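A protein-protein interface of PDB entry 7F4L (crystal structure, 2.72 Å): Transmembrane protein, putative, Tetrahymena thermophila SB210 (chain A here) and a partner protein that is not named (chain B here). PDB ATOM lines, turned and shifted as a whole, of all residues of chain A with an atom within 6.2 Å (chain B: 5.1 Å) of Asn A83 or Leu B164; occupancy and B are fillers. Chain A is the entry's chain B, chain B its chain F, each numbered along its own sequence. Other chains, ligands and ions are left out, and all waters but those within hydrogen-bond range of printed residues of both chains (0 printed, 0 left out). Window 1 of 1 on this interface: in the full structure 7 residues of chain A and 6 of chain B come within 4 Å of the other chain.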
ATOM      1  N   GLN A  48      13.289  32.132 -10.569  1.00  0.00           N
ATOM      2  CA  GLN A  48      13.537  32.098 -11.999  1.00  0.00           C
ATOM      3  C   GLN A  48      14.874  32.707 -12.394  1.00  0.00           C
ATOM      4  O   GLN A  48      15.018  33.183 -13.516  1.00  0.00           O
ATOM      5  CB  GLN A  48      12.424  32.820 -12.740  1.00  0.00           C
ATOM      6  CG  GLN A  48      11.054  32.473 -12.288  1.00  0.00           C
ATOM      7  CD  GLN A  48      10.019  33.003 -13.228  1.00  0.00           C
ATOM      8  OE1 GLN A  48      10.307  33.824 -14.104  1.00  0.00           O
ATOM      9  NE2 GLN A  48       8.802  32.565 -13.043  1.00  0.00           N
ATOM     10  N   ASN A  74      17.608  18.726 -20.015  1.00  0.00           N
ATOM     11  CA  ASN A  74      17.080  18.975 -18.684  1.00  0.00           C
ATOM     12  C   ASN A  74      17.435  17.839 -17.754  1.00  0.00           C
ATOM     13  O   ASN A  74      17.866  18.056 -16.624  1.00  0.00           O
ATOM     14  CB  ASN A  74      15.575  19.168 -18.748  1.00  0.00           C
ATOM     15  CG  ASN A  74      15.018  19.830 -17.520  1.00  0.00           C
ATOM     16  OD1 ASN A  74      15.690  20.564 -16.836  1.00  0.00           O
ATOM     17  ND2 ASN A  74      13.774  19.556 -17.237  1.00  0.00           N
ATOM     18  N   LYS A  81      15.298  20.225 -13.425  1.00  0.00           N
ATOM     19  CA  LYS A  81      14.697  21.365 -12.782  1.00  0.00           C
ATOM     20  C   LYS A  81      14.618  22.637 -13.611  1.00  0.00           C
ATOM     21  O   LYS A  81      14.056  23.600 -13.158  1.00  0.00           O
ATOM     22  CB  LYS A  81      15.409  21.618 -11.450  1.00  0.00           C
ATOM     23  CG  LYS A  81      14.785  20.951 -10.237  1.00  0.00           C
ATOM     24  CD  LYS A  81      14.418  19.502 -10.471  1.00  0.00           C
ATOM     25  CE  LYS A  81      12.948  19.255 -10.194  1.00  0.00           C
ATOM     26  NZ  LYS A  81      12.401  18.056 -10.886  1.00  0.00           N
ATOM     27  N   ALA A  82      15.153  22.643 -14.823  1.00  0.00           N
ATOM     28  CA  ALA A  82      15.046  23.819 -15.659  1.00  0.00           C
ATOM     29  C   ALA A  82      13.676  23.913 -16.326  1.00  0.00           C
ATOM     30  O   ALA A  82      12.849  23.000 -16.293  1.00  0.00           O
ATOM     31  CB  ALA A  82      16.120  23.826 -16.732  1.00  0.00           C
ATOM     32  N   ASN A  83      13.468  25.053 -16.959  1.00  0.00           N
ATOM     33  CA  ASN A  83      12.297  25.331 -17.761  1.00  0.00           C
ATOM     34  C   ASN A  83      12.622  25.002 -19.208  1.00  0.00           C
ATOM     35  O   ASN A  83      13.538  25.581 -19.785  1.00  0.00           O
ATOM     36  CB  ASN A  83      11.945  26.798 -17.598  1.00  0.00           C
ATOM     37  CG  ASN A  83      10.639  27.153 -18.209  1.00  0.00           C
ATOM     38  OD1 ASN A  83      10.061  26.381 -18.966  1.00  0.00           O
ATOM     39  ND2 ASN A  83      10.159  28.347 -17.898  1.00  0.00           N
ATOM     40  N   ILE A  84      11.869  24.078 -19.789  1.00  0.00           N
ATOM     41  CA  ILE A  84      12.147  23.633 -21.144  1.00  0.00           C
ATOM     42  C   ILE A  84      12.022  24.784 -22.120  1.00  0.00           C
ATOM     43  O   ILE A  84      12.825  24.912 -23.043  1.00  0.00           O
ATOM     44  CB  ILE A  84      11.222  22.463 -21.496  1.00  0.00           C
ATOM     45  CG1 ILE A  84      12.054  21.395 -22.119  1.00  0.00           C
ATOM     46  CG2 ILE A  84      10.182  22.834 -22.509  1.00  0.00           C
ATOM     47  CD1 ILE A  84      13.072  20.967 -21.172  1.00  0.00           C
ATOM     48  N   VAL A  85      11.041  25.664 -21.908  1.00  0.00           N
ATOM     49  CA  VAL A  85      10.890  26.836 -22.752  1.00  0.00           C
ATOM     50  C   VAL A  85      12.067  27.778 -22.566  1.00  0.00           C
ATOM     51  O   VAL A  85      12.613  28.322 -23.518  1.00  0.00           O
ATOM     52  CB  VAL A  85       9.558  27.526 -22.434  1.00  0.00           C
ATOM     53  CG1 VAL A  85       9.398  28.752 -23.311  1.00  0.00           C
ATOM     54  CG2 VAL A  85       8.396  26.569 -22.652  1.00  0.00           C
ATOM     55  N   GLU A  86      12.475  27.996 -21.343  1.00  0.00           N
ATOM     56  CA  GLU A  86      13.628  28.844 -21.124  1.00  0.00           C
ATOM     57  C   GLU A  86      14.849  28.330 -21.854  1.00  0.00           C
ATOM     58  O   GLU A  86      15.616  29.111 -22.418  1.00  0.00           O
ATOM     59  CB  GLU A  86      13.888  28.920 -19.642  1.00  0.00           C
ATOM     60  CG  GLU A  86      14.860  29.891 -19.326  1.00  0.00           C
ATOM     61  CD  GLU A  86      15.059  30.165 -17.876  1.00  0.00           C
ATOM     62  OE1 GLU A  86      14.592  29.412 -17.051  1.00  0.00           O
ATOM     63  OE2 GLU A  86      15.587  31.215 -17.439  1.00  0.00           O
ATOM     64  N   LEU A  87      15.049  27.018 -21.847  1.00  0.00           N
ATOM     65  CA  LEU A  87      16.135  26.427 -22.600  1.00  0.00           C
ATOM     66  C   LEU A  87      16.062  26.824 -24.061  1.00  0.00           C
ATOM     67  O   LEU A  87      16.990  27.420 -24.594  1.00  0.00           O
ATOM     68  CB  LEU A  87      16.073  24.923 -22.436  1.00  0.00           C
ATOM     69  CG  LEU A  87      16.396  24.530 -21.014  1.00  0.00           C
ATOM     70  CD1 LEU A  87      16.381  23.040 -20.826  1.00  0.00           C
ATOM     71  CD2 LEU A  87      17.720  25.112 -20.656  1.00  0.00           C
ATOM     72  N   GLU A  88      14.937  26.534 -24.707  1.00  0.00           N
ATOM     73  CA  GLU A  88      14.730  26.928 -26.096  1.00  0.00           C
ATOM     74  C   GLU A  88      15.054  28.399 -26.331  1.00  0.00           C
ATOM     75  O   GLU A  88      15.649  28.750 -27.347  1.00  0.00           O
ATOM     76  CB  GLU A  88      13.283  26.658 -26.501  1.00  0.00           C
ATOM     77  CG  GLU A  88      13.100  25.908 -27.779  1.00  0.00           C
ATOM     78  CD  GLU A  88      12.329  26.651 -28.811  1.00  0.00           C
ATOM     79  OE1 GLU A  88      12.529  27.870 -28.895  1.00  0.00           O
ATOM     80  OE2 GLU A  88      11.545  26.033 -29.560  1.00  0.00           O
ATOM     81  N   LEU A  89      14.648  29.279 -25.418  1.00  0.00           N
ATOM     82  CA  LEU A  89      14.817  30.707 -25.641  1.00  0.00           C
ATOM     83  C   LEU A  89      16.262  31.132 -25.504  1.00  0.00           C
ATOM     84  O   LEU A  89      16.736  31.970 -26.274  1.00  0.00           O
ATOM     85  CB  LEU A  89      13.969  31.499 -24.655  1.00  0.00           C
ATOM     86  CG  LEU A  89      12.455  31.552 -24.819  1.00  0.00           C
ATOM     87  CD1 LEU A  89      11.918  32.363 -23.694  1.00  0.00           C
ATOM     88  CD2 LEU A  89      12.079  32.157 -26.143  1.00  0.00           C
ATOM     89  N   ARG A  90      16.923  30.550 -24.531  1.00  0.00           N
ATOM     90  CA  ARG A  90      18.287  30.823 -24.214  1.00  0.00           C
ATOM     91  C   ARG A  90      19.201  30.464 -25.358  1.00  0.00           C
ATOM     92  O   ARG A  90      20.254  31.044 -25.472  1.00  0.00           O
ATOM     93  CB  ARG A  90      18.659  30.033 -22.980  1.00  0.00           C
ATOM     94  CG  ARG A  90      19.001  30.873 -21.784  1.00  0.00           C
ATOM     95  CD  ARG A  90      17.822  31.584 -21.216  1.00  0.00           C
ATOM     96  NE  ARG A  90      18.261  32.820 -20.628  1.00  0.00           N
ATOM     97  CZ  ARG A  90      17.716  33.369 -19.573  1.00  0.00           C
ATOM     98  NH1 ARG A  90      16.705  32.785 -18.992  1.00  0.00           N
ATOM     99  NH2 ARG A  90      18.173  34.493 -19.112  1.00  0.00           N
ATOM    100  N   THR B 162       5.413  37.359 -16.096  1.00  0.00           N
ATOM    101  CA  THR B 162       6.606  37.850 -16.758  1.00  0.00           C
ATOM    102  C   THR B 162       6.660  37.326 -18.183  1.00  0.00           C
ATOM    103  O   THR B 162       5.909  36.438 -18.579  1.00  0.00           O
ATOM    104  CB  THR B 162       7.858  37.439 -15.990  1.00  0.00           C
ATOM    105  OG1 THR B 162       8.275  36.144 -16.416  1.00  0.00           O
ATOM    106  CG2 THR B 162       7.550  37.351 -14.552  1.00  0.00           C
ATOM    107  N   ASN B 163       7.564  37.900 -18.966  1.00  0.00           N
ATOM    108  CA  ASN B 163       7.702  37.481 -20.352  1.00  0.00           C
ATOM    109  C   ASN B 163       7.914  35.984 -20.459  1.00  0.00           C
ATOM    110  O   ASN B 163       7.383  35.344 -21.362  1.00  0.00           O
ATOM    111  CB  ASN B 163       8.855  38.220 -21.003  1.00  0.00           C
ATOM    112  CG  ASN B 163       8.520  39.633 -21.313  1.00  0.00           C
ATOM    113  OD1 ASN B 163       7.454  39.928 -21.821  1.00  0.00           O
ATOM    114  ND2 ASN B 163       9.423  40.535 -20.977  1.00  0.00           N
ATOM    115  N   LEU B 164       8.683  35.412 -19.544  1.00  0.00           N
ATOM    116  CA  LEU B 164       8.991  33.995 -19.594  1.00  0.00           C
ATOM    117  C   LEU B 164       7.815  33.155 -19.173  1.00  0.00           C
ATOM    118  O   LEU B 164       7.610  32.078 -19.716  1.00  0.00           O
ATOM    119  CB  LEU B 164      10.171  33.682 -18.684  1.00  0.00           C
ATOM    120  CG  LEU B 164      11.215  32.599 -18.966  1.00  0.00           C
ATOM    121  CD1 LEU B 164      11.804  32.180 -17.692  1.00  0.00           C
ATOM    122  CD2 LEU B 164      10.710  31.412 -19.694  1.00  0.00           C
ATOM    123  N   GLU B 165       7.049  33.607 -18.196  1.00  0.00           N
ATOM    124  CA  GLU B 165       5.848  32.875 -17.823  1.00  0.00           C
ATOM    125  C   GLU B 165       4.832  32.886 -18.954  1.00  0.00           C
ATOM    126  O   GLU B 165       4.211  31.865 -19.252  1.00  0.00           O
ATOM    127  CB  GLU B 165       5.257  33.474 -16.551  1.00  0.00           C
ATOM    128  CG  GLU B 165       6.223  33.506 -15.413  1.00  0.00           C
ATOM    129  CD  GLU B 165       5.666  34.193 -14.215  1.00  0.00           C
ATOM    130  OE1 GLU B 165       5.067  35.272 -14.376  1.00  0.00           O
ATOM    131  OE2 GLU B 165       5.835  33.669 -13.103  1.00  0.00           O
ATOM    132  N   ILE B 166       4.647  34.032 -19.591  1.00  0.00           N
ATOM    133  CA  ILE B 166       3.726  34.099 -20.710  1.00  0.00           C
ATOM    134  C   ILE B 166       4.138  33.109 -21.781  1.00  0.00           C
ATOM    135  O   ILE B 166       3.331  32.304 -22.246  1.00  0.00           O
ATOM    136  CB  ILE B 166       3.670  35.530 -21.255  1.00  0.00           C
ATOM    137  CG1 ILE B 166       3.131  36.481 -20.200  1.00  0.00           C
ATOM    138  CG2 ILE B 166       2.845  35.571 -22.488  1.00  0.00           C
ATOM    139  CD1 ILE B 166       3.283  37.889 -20.563  1.00  0.00           C
ATOM    140  N   LEU B 167       5.412  33.143 -22.173  1.00  0.00           N
ATOM    141  CA  LEU B 167       5.909  32.237 -23.197  1.00  0.00           C
ATOM    142  C   LEU B 167       5.738  30.778 -22.811  1.00  0.00           C
ATOM    143  O   LEU B 167       5.431  29.950 -23.672  1.00  0.00           O
ATOM    144  CB  LEU B 167       7.364  32.535 -23.492  1.00  0.00           C
ATOM    145  CG  LEU B 167       7.526  33.794 -24.327  1.00  0.00           C
ATOM    146  CD1 LEU B 167       8.883  34.346 -24.173  1.00  0.00           C
ATOM    147  CD2 LEU B 167       7.260  33.509 -25.761  1.00  0.00           C
ATOM    148  N   THR B 168       5.905  30.446 -21.538  1.00  0.00           N
ATOM    149  CA  THR B 168       5.672  29.075 -21.104  1.00  0.00           C
ATOM    150  C   THR B 168       4.210  28.673 -21.277  1.00  0.00           C
ATOM    151  O   THR B 168       3.920  27.578 -21.761  1.00  0.00           O
ATOM    152  CB  THR B 168       6.118  28.901 -19.656  1.00  0.00           C
ATOM    153  OG1 THR B 168       7.449  29.378 -19.498  1.00  0.00           O
ATOM    154  CG2 THR B 168       6.093  27.483 -19.289  1.00  0.00           C
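Among the printed residues, merely in contact across the chains: Gln A48 with Thr B162, Asn A83 with Leu B164, Glu A86 with Leu B164 and Leu A89 with Leu B167.
The side-chain amide nitrogen (NE2) of Gln A48 sits at hydrogen-bond distance from the side-chain carboxylate (OE2) of Glu B165, at 3.2 Å.
ND2 of Asn A83 is in hydrogen-bond range of OG1 of Thr B168 (3.3 Å).
The side-chain amide oxygen of Asn A83 sits at hydrogen-bond distance from the backbone NH of Val A85, 3.2 Å away.
NH1 of Arg A90 lies within salt-bridge range of OE2 of Glu A86 (2.5 Å).
The backbone NH of Leu B164 sits close to the side-chain hydroxyl of Thr B162.
N of Thr B162 sits at hydrogen-bond distance from OE1 of Glu B165, at 2.7 Å.
The side-chain hydroxyl (OG1) of Thr B168 is in hydrogen-bond range of the backbone carbonyl oxygen (O) of Leu B164 (2.7 Å).
Printed residues of chain B within 4 Å of Glu A86: Leu B164 (3.8 Å).
Leu A87 touches none of the printed residues of chain B.
Asn B163 touches none of the printed residues of chain A.
Of chain A, only Asn A83 (3.6 Å) and Glu A86 (3.8 Å) come within 4 Å of Leu B164.
Of the printed residues of chain A, Glu B165 touches Gln A48 (3.2 Å).
The nearest printed residue of chain B that does not touch Asn A83 is Glu B165 (6.1 Å).
The nearest residue of chain A that does not touch Leu B164 is Gln A48 (4.2 Å).
The nearest printed residue of chain B that does not touch Leu A89 is Leu B164 (4.3 Å).
Hydrophobic or aromatic side chains of chain A that line the printed part of chain B: Leu A89.
Of the 7 printed residues of chain B, 5 touch a printed residue of chain A.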
